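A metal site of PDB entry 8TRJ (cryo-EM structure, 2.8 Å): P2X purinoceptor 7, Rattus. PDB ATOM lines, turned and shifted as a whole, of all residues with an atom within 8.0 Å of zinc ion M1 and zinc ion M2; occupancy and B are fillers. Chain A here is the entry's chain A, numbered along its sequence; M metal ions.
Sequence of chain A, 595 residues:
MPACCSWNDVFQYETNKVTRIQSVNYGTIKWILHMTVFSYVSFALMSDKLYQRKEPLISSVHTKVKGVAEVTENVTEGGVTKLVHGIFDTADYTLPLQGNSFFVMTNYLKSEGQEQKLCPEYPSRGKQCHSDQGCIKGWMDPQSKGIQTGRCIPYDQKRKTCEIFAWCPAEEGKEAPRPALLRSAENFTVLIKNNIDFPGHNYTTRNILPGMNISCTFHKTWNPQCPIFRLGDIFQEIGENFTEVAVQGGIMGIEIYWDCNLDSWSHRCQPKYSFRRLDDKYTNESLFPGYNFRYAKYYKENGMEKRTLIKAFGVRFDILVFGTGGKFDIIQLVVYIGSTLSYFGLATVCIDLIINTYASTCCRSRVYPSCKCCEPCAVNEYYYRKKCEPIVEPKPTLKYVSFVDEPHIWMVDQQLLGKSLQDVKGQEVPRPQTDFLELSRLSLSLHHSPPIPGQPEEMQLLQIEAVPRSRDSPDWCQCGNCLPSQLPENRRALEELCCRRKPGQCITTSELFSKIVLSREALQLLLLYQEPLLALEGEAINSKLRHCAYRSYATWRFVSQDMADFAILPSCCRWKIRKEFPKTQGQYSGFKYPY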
ATOM      1  N   VAL A 404       1.621   6.707  19.629  1.00  0.00           N
ATOM      2  CA  VAL A 404       2.385   7.066  20.815  1.00  0.00           C
ATOM      3  C   VAL A 404       3.503   8.002  20.415  1.00  0.00           C
ATOM      4  O   VAL A 404       3.726   9.033  21.055  1.00  0.00           O
ATOM      5  CB  VAL A 404       2.975   5.826  21.510  1.00  0.00           C
ATOM      6  CG1 VAL A 404       3.847   6.240  22.670  1.00  0.00           C
ATOM      7  CG2 VAL A 404       1.875   4.893  21.975  1.00  0.00           C
ATOM      8  N   GLN A 422      -3.510   3.063   8.577  1.00  0.00           N
ATOM      9  CA  GLN A 422      -2.148   3.423   8.934  1.00  0.00           C
ATOM     10  C   GLN A 422      -1.518   4.315   7.873  1.00  0.00           C
ATOM     11  O   GLN A 422      -0.942   5.366   8.178  1.00  0.00           O
ATOM     12  CB  GLN A 422      -1.314   2.163   9.134  1.00  0.00           C
ATOM     13  CG  GLN A 422       0.171   2.380   9.385  1.00  0.00           C
ATOM     14  CD  GLN A 422       0.461   2.937  10.759  1.00  0.00           C
ATOM     15  OE1 GLN A 422       0.202   2.286  11.778  1.00  0.00           O
ATOM     16  NE2 GLN A 422       1.019   4.139  10.801  1.00  0.00           N
ATOM     17  N   SER A 473       4.111  -9.382  12.296  1.00  0.00           N
ATOM     18  CA  SER A 473       4.410  -7.984  11.965  1.00  0.00           C
ATOM     19  C   SER A 473       3.918  -7.642  10.568  1.00  0.00           C
ATOM     20  O   SER A 473       4.689  -7.690   9.612  1.00  0.00           O
ATOM     21  CB  SER A 473       5.903  -7.710  12.082  1.00  0.00           C
ATOM     22  OG  SER A 473       6.379  -7.978  13.387  1.00  0.00           O
ATOM     23  N   PRO A 474       2.633  -7.281  10.441  1.00  0.00           N
ATOM     24  CA  PRO A 474       2.128  -6.826   9.134  1.00  0.00           C
ATOM     25  C   PRO A 474       2.974  -5.707   8.541  1.00  0.00           C
ATOM     26  O   PRO A 474       3.753  -5.057   9.259  1.00  0.00           O
ATOM     27  CB  PRO A 474       0.709  -6.354   9.469  1.00  0.00           C
ATOM     28  CG  PRO A 474       0.344  -7.118  10.675  1.00  0.00           C
ATOM     29  CD  PRO A 474       1.597  -7.243  11.472  1.00  0.00           C
ATOM     30  N   TRP A 476       2.280  -2.836   7.734  1.00  0.00           N
ATOM     31  CA  TRP A 476       1.981  -1.548   8.361  1.00  0.00           C
ATOM     32  C   TRP A 476       2.289  -1.524   9.844  1.00  0.00           C
ATOM     33  O   TRP A 476       2.052  -0.504  10.503  1.00  0.00           O
ATOM     34  CB  TRP A 476       0.511  -1.181   8.141  1.00  0.00           C
ATOM     35  CG  TRP A 476      -0.465  -2.300   8.309  1.00  0.00           C
ATOM     36  CD1 TRP A 476      -1.117  -2.966   7.324  1.00  0.00           C
ATOM     37  CD2 TRP A 476      -0.892  -2.882   9.551  1.00  0.00           C
ATOM     38  NE1 TRP A 476      -1.936  -3.929   7.869  1.00  0.00           N
ATOM     39  CE2 TRP A 476      -1.811  -3.900   9.236  1.00  0.00           C
ATOM     40  CE3 TRP A 476      -0.590  -2.639  10.894  1.00  0.00           C
ATOM     41  CZ2 TRP A 476      -2.434  -4.680  10.205  1.00  0.00           C
ATOM     42  CZ3 TRP A 476      -1.201  -3.418  11.854  1.00  0.00           C
ATOM     43  CH2 TRP A 476      -2.118  -4.417  11.506  1.00  0.00           C
ATOM     44  N   CYS A 477       2.828  -2.607  10.403  1.00  0.00           N
ATOM     45  CA  CYS A 477       3.073  -2.709  11.835  1.00  0.00           C
ATOM     46  C   CYS A 477       4.503  -2.327  12.169  1.00  0.00           C
ATOM     47  O   CYS A 477       5.451  -2.821  11.546  1.00  0.00           O
ATOM     48  CB  CYS A 477       2.785  -4.118  12.329  1.00  0.00           C
ATOM     49  SG  CYS A 477       3.151  -4.373  14.074  1.00  0.00           S
ATOM     50  N   GLN A 478       4.653  -1.439  13.154  1.00  0.00           N
ATOM     51  CA  GLN A 478       5.958  -1.056  13.679  1.00  0.00           C
ATOM     52  C   GLN A 478       6.199  -1.584  15.084  1.00  0.00           C
ATOM     53  O   GLN A 478       7.315  -1.432  15.604  1.00  0.00           O
ATOM     54  CB  GLN A 478       6.095   0.470  13.686  1.00  0.00           C
ATOM     55  CG  GLN A 478       6.454   1.078  12.345  1.00  0.00           C
ATOM     56  CD  GLN A 478       5.262   1.170  11.398  1.00  0.00           C
ATOM     57  OE1 GLN A 478       4.461   0.250  11.299  1.00  0.00           O
ATOM     58  NE2 GLN A 478       5.161   2.292  10.691  1.00  0.00           N
ATOM     59  N   CYS A 479       5.200  -2.189  15.721  1.00  0.00           N
ATOM     60  CA  CYS A 479       5.324  -2.692  17.083  1.00  0.00           C
ATOM     61  C   CYS A 479       5.511  -4.203  17.149  1.00  0.00           C
ATOM     62  O   CYS A 479       6.137  -4.695  18.104  1.00  0.00           O
ATOM     63  CB  CYS A 479       4.096  -2.308  17.899  1.00  0.00           C
ATOM     64  SG  CYS A 479       2.657  -3.376  17.650  1.00  0.00           S
ATOM     65  N   GLY A 480       4.995  -4.943  16.180  1.00  0.00           N
ATOM     66  CA  GLY A 480       5.167  -6.375  16.105  1.00  0.00           C
ATOM     67  C   GLY A 480       4.049  -7.192  16.726  1.00  0.00           C
ATOM     68  O   GLY A 480       3.927  -8.381  16.407  1.00  0.00           O
ATOM     69  N   ASN A 481       3.225  -6.593  17.587  1.00  0.00           N
ATOM     70  CA  ASN A 481       2.131  -7.312  18.213  1.00  0.00           C
ATOM     71  C   ASN A 481       0.829  -7.203  17.431  1.00  0.00           C
ATOM     72  O   ASN A 481      -0.158  -7.846  17.819  1.00  0.00           O
ATOM     73  CB  ASN A 481       1.906  -6.789  19.635  1.00  0.00           C
ATOM     74  CG  ASN A 481       1.029  -7.717  20.460  1.00  0.00           C
ATOM     75  OD1 ASN A 481       0.701  -8.822  20.023  1.00  0.00           O
ATOM     76  ND2 ASN A 481       0.661  -7.288  21.655  1.00  0.00           N
ATOM     77  N   CYS A 482       0.797  -6.426  16.360  1.00  0.00           N
ATOM     78  CA  CYS A 482      -0.419  -6.305  15.567  1.00  0.00           C
ATOM     79  C   CYS A 482      -0.714  -7.601  14.839  1.00  0.00           C
ATOM     80  O   CYS A 482       0.154  -8.153  14.159  1.00  0.00           O
ATOM     81  CB  CYS A 482      -0.299  -5.161  14.571  1.00  0.00           C
ATOM     82  SG  CYS A 482      -0.331  -3.507  15.314  1.00  0.00           S
ATOM     83  N   LEU A 483      -1.933  -8.106  14.977  1.00  0.00           N
ATOM     84  CA  LEU A 483      -2.346  -9.302  14.272  1.00  0.00           C
ATOM     85  C   LEU A 483      -3.105  -8.912  13.015  1.00  0.00           C
ATOM     86  O   LEU A 483      -3.859  -7.924  13.033  1.00  0.00           O
ATOM     87  CB  LEU A 483      -3.234 -10.174  15.147  1.00  0.00           C
ATOM     88  CG  LEU A 483      -2.792 -10.453  16.576  1.00  0.00           C
ATOM     89  CD1 LEU A 483      -3.703 -11.485  17.207  1.00  0.00           C
ATOM     90  CD2 LEU A 483      -1.340 -10.916  16.639  1.00  0.00           C
ATOM     91  N   LEU A 497      -3.871  -0.816  11.490  1.00  0.00           N
ATOM     92  CA  LEU A 497      -3.334   0.302  12.256  1.00  0.00           C
ATOM     93  C   LEU A 497      -2.361  -0.217  13.302  1.00  0.00           C
ATOM     94  O   LEU A 497      -2.524  -1.309  13.840  1.00  0.00           O
ATOM     95  CB  LEU A 497      -4.470   1.093  12.928  1.00  0.00           C
ATOM     96  CG  LEU A 497      -4.089   2.357  13.715  1.00  0.00           C
ATOM     97  CD1 LEU A 497      -3.485   3.492  12.897  1.00  0.00           C
ATOM     98  CD2 LEU A 497      -5.189   2.826  14.663  1.00  0.00           C
ATOM     99  N   CYS A 498      -1.344   0.596  13.594  1.00  0.00           N
ATOM    100  CA  CYS A 498      -0.330   0.270  14.576  1.00  0.00           C
ATOM    101  C   CYS A 498      -0.326   1.317  15.687  1.00  0.00           C
ATOM    102  O   CYS A 498      -0.671   2.478  15.464  1.00  0.00           O
ATOM    103  CB  CYS A 498       1.066   0.198  13.952  1.00  0.00           C
ATOM    104  SG  CYS A 498       2.257  -0.763  14.893  1.00  0.00           S
ATOM    105  N   CYS A 499       0.070   0.879  16.875  1.00  0.00           N
ATOM    106  CA  CYS A 499       0.101   1.779  18.024  1.00  0.00           C
ATOM    107  C   CYS A 499       1.047   2.954  17.805  1.00  0.00           C
ATOM    108  O   CYS A 499       0.856   4.022  18.384  1.00  0.00           O
ATOM    109  CB  CYS A 499       0.503   1.010  19.271  1.00  0.00           C
ATOM    110  SG  CYS A 499       2.004   0.050  19.078  1.00  0.00           S
ATOM    111  N   ARG A 500       2.083   2.759  16.986  1.00  0.00           N
ATOM    112  CA  ARG A 500       3.057   3.813  16.710  1.00  0.00           C
ATOM    113  C   ARG A 500       3.372   3.834  15.224  1.00  0.00           C
ATOM    114  O   ARG A 500       3.236   2.820  14.523  1.00  0.00           O
ATOM    115  CB  ARG A 500       4.347   3.622  17.519  1.00  0.00           C
ATOM    116  CG  ARG A 500       4.899   2.209  17.498  1.00  0.00           C
ATOM    117  CD  ARG A 500       6.002   2.044  18.523  1.00  0.00           C
ATOM    118  NE  ARG A 500       6.832   3.249  18.660  1.00  0.00           N
ATOM    119  CZ  ARG A 500       7.473   3.606  19.768  1.00  0.00           C
ATOM    120  NH1 ARG A 500       7.403   2.865  20.854  1.00  0.00           N
ATOM    121  NH2 ARG A 500       8.193   4.712  19.777  1.00  0.00           N
ATOM    122  N   GLY A 504       9.444   0.681  17.671  1.00  0.00           N
ATOM    123  CA  GLY A 504       9.721   0.963  19.067  1.00  0.00           C
ATOM    124  C   GLY A 504       8.886   0.077  19.957  1.00  0.00           C
ATOM    125  O   GLY A 504       8.274  -0.902  19.517  1.00  0.00           O
ATOM    126  N   GLN A 505       8.879   0.436  21.246  1.00  0.00           N
ATOM    127  CA  GLN A 505       8.114  -0.321  22.223  1.00  0.00           C
ATOM    128  C   GLN A 505       6.616  -0.178  21.957  1.00  0.00           C
ATOM    129  O   GLN A 505       6.127   0.917  21.658  1.00  0.00           O
ATOM    130  CB  GLN A 505       8.452   0.154  23.634  1.00  0.00           C
ATOM    131  CG  GLN A 505       9.592  -0.617  24.279  1.00  0.00           C
ATOM    132  CD  GLN A 505       9.824  -0.204  25.721  1.00  0.00           C
ATOM    133  OE1 GLN A 505       9.151   0.682  26.247  1.00  0.00           O
ATOM    134  NE2 GLN A 505      10.801  -0.835  26.365  1.00  0.00           N
ATOM    135  N   CYS A 506       5.903  -1.286  22.071  1.00  0.00           N
ATOM    136  CA  CYS A 506       4.456  -1.276  21.880  1.00  0.00           C
ATOM    137  C   CYS A 506       3.770  -0.602  23.058  1.00  0.00           C
ATOM    138  O   CYS A 506       4.192  -0.743  24.207  1.00  0.00           O
ATOM    139  CB  CYS A 506       3.941  -2.698  21.708  1.00  0.00           C
ATOM    140  SG  CYS A 506       2.175  -2.822  21.332  1.00  0.00           S
ATOM    141  N   ILE A 507       2.699   0.141  22.772  1.00  0.00           N
ATOM    142  CA  ILE A 507       1.874   0.685  23.838  1.00  0.00           C
ATOM    143  C   ILE A 507       1.263  -0.438  24.659  1.00  0.00           C
ATOM    144  O   ILE A 507       0.995  -0.278  25.854  1.00  0.00           O
ATOM    145  CB  ILE A 507       0.784   1.601  23.265  1.00  0.00           C
ATOM    146  CG1 ILE A 507       0.213   2.503  24.352  1.00  0.00           C
ATOM    147  CG2 ILE A 507      -0.328   0.777  22.673  1.00  0.00           C
ATOM    148  CD1 ILE A 507      -0.727   3.555  23.832  1.00  0.00           C
ATOM    149  N   THR A 508       1.033  -1.595  24.036  1.00  0.00           N
ATOM    150  CA  THR A 508       0.340  -2.685  24.704  1.00  0.00           C
ATOM    151  C   THR A 508       1.107  -3.184  25.915  1.00  0.00           C
ATOM    152  O   THR A 508       0.515  -3.545  26.935  1.00  0.00           O
ATOM    153  CB  THR A 508       0.090  -3.818  23.717  1.00  0.00           C
ATOM    154  OG1 THR A 508      -0.657  -3.322  22.598  1.00  0.00           O
ATOM    155  CG2 THR A 508      -0.684  -4.926  24.365  1.00  0.00           C
ATOM    156  N   THR A 509       2.444  -3.219  25.818  1.00  0.00           N
ATOM    157  CA  THR A 509       3.253  -3.663  26.943  1.00  0.00           C
ATOM    158  C   THR A 509       3.346  -2.628  28.044  1.00  0.00           C
ATOM    159  O   THR A 509       3.885  -2.923  29.114  1.00  0.00           O
ATOM    160  CB  THR A 509       4.662  -4.047  26.476  1.00  0.00           C
ATOM    161  OG1 THR A 509       5.462  -4.397  27.608  1.00  0.00           O
ATOM    162  CG2 THR A 509       5.319  -2.890  25.724  1.00  0.00           C
ATOM    163  N   TYR A 553      -9.481   2.744  26.274  1.00  0.00           N
ATOM    164  CA  TYR A 553      -8.398   3.167  25.396  1.00  0.00           C
ATOM    165  C   TYR A 553      -8.763   4.462  24.681  1.00  0.00           C
ATOM    166  O   TYR A 553      -7.977   5.417  24.673  1.00  0.00           O
ATOM    167  CB  TYR A 553      -8.063   2.069  24.386  1.00  0.00           C
ATOM    168  CG  TYR A 553      -6.854   2.372  23.545  1.00  0.00           C
ATOM    169  CD1 TYR A 553      -6.964   3.075  22.356  1.00  0.00           C
ATOM    170  CD2 TYR A 553      -5.590   1.985  23.951  1.00  0.00           C
ATOM    171  CE1 TYR A 553      -5.864   3.360  21.592  1.00  0.00           C
ATOM    172  CE2 TYR A 553      -4.478   2.268  23.193  1.00  0.00           C
ATOM    173  CZ  TYR A 553      -4.625   2.954  22.010  1.00  0.00           C
ATOM    174  OH  TYR A 553      -3.516   3.244  21.247  1.00  0.00           O
ATOM    175  N   PRO A 570      -5.730   0.480  17.573  1.00  0.00           N
ATOM    176  CA  PRO A 570      -4.741  -0.292  16.814  1.00  0.00           C
ATOM    177  C   PRO A 570      -5.018  -1.784  16.906  1.00  0.00           C
ATOM    178  O   PRO A 570      -5.708  -2.266  17.813  1.00  0.00           O
ATOM    179  CB  PRO A 570      -3.420   0.071  17.486  1.00  0.00           C
ATOM    180  CG  PRO A 570      -3.672   1.332  18.192  1.00  0.00           C
ATOM    181  CD  PRO A 570      -5.091   1.281  18.624  1.00  0.00           C
ATOM    182  N   SER A 571      -4.477  -2.507  15.939  1.00  0.00           N
ATOM    183  CA  SER A 571      -4.708  -3.948  15.878  1.00  0.00           C
ATOM    184  C   SER A 571      -4.149  -4.648  17.120  1.00  0.00           C
ATOM    185  O   SER A 571      -4.798  -5.544  17.667  1.00  0.00           O
ATOM    186  CB  SER A 571      -4.089  -4.521  14.611  1.00  0.00           C
ATOM    187  OG  SER A 571      -4.499  -5.860  14.398  1.00  0.00           O
ATOM    188  N   CYS A 572      -2.965  -4.250  17.571  1.00  0.00           N
ATOM    189  CA  CYS A 572      -2.347  -4.923  18.713  1.00  0.00           C
ATOM    190  C   CYS A 572      -3.236  -4.817  19.951  1.00  0.00           C
ATOM    191  O   CYS A 572      -3.538  -5.821  20.607  1.00  0.00           O
ATOM    192  CB  CYS A 572      -0.969  -4.329  18.988  1.00  0.00           C
ATOM    193  SG  CYS A 572      -0.894  -2.523  19.038  1.00  0.00           S
ATOM    194  N   CYS A 573      -3.653  -3.601  20.289  1.00  0.00           N
ATOM    195  CA  CYS A 573      -4.482  -3.394  21.472  1.00  0.00           C
ATOM    196  C   CYS A 573      -5.835  -4.083  21.327  1.00  0.00           C
ATOM    197  O   CYS A 573      -6.316  -4.726  22.263  1.00  0.00           O
ATOM    198  CB  CYS A 573      -4.667  -1.894  21.708  1.00  0.00           C
ATOM    199  SG  CYS A 573      -3.154  -0.948  21.432  1.00  0.00           S
HETATM  200 ZN    ZN M   1       1.920  -2.986  15.477  1.00  0.00          ZN
HETATM  201 ZN    ZN M   2       1.411  -2.195  19.227  1.00  0.00          ZN
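OE1 of Gln 422 is in hydrogen-bond range of N of Cys 498, at 2.9 Å. O of Leu 497 sits close to SG of Cys 482 (3.4 Å). The side-chain sulfur of Cys 477 lies close to the backbone NH of Gly 480, 2.9 Å away. The side-chain sulfur (SG) of Cys 482 lies close to the backbone NH (N) of Cys 572, 3.5 Å away. The side-chain sulfur of Cys 479 sits close to the backbone NH of Asn 481 (3.3 Å). The side-chain sulfur (SG) of Cys 572 lies close to the side-chain hydroxyl (OG1) of Thr 508 (3.7 Å). The side-chain sulfur (SG) of Cys 498 lies close to the backbone NH (N) of Gln 478 (3.0 Å). The backbone carbonyl oxygen (O) of Arg 500 lies close to the side-chain sulfur (SG) of Cys 498 (3.7 Å).
Merely in contact with zinc ion M1: Gln 478 (3.9 Å) and Gly 480 (3.7 Å). Six residues have an atom within 4 Å of zinc ion M1: Cys 477, Gln 478, Cys 479, Gly 480, Cys 482 and Cys 498. Along chain A the residues within 4 Å of zinc ion M1 span positions 477 to 498.
Within 4 Å of zinc ion M2: Cys 479, Cys 499, Cys 506 and Cys 572. The nearest printed residue that does not touch zinc ion M2 is Thr 508 (4.1 Å).
Zinc ion M1 is bound by the side-chain sulfur of Cys 482 (2.3 Å), the side-chain sulfur of Cys 498 (2.3 Å), the side-chain sulfur of Cys 477 (2.3 Å) and the side-chain sulfur of Cys 479 (2.3 Å). Zinc ion M1 has four donor atoms within binding distance.
SG of Cys 506 is bound to zinc ion M2, 2.3 Å away. Zinc ion M2 is bound by SG of Cys 499 (2.3 Å). The side-chain sulfur (SG) of Cys 479 binds zinc ion M2 (2.3 Å). Zinc ion M2 is bound by the side-chain sulfur (SG) of Cys 572, at 2.3 Å. Zinc ion M2 has four donor atoms within binding distance.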
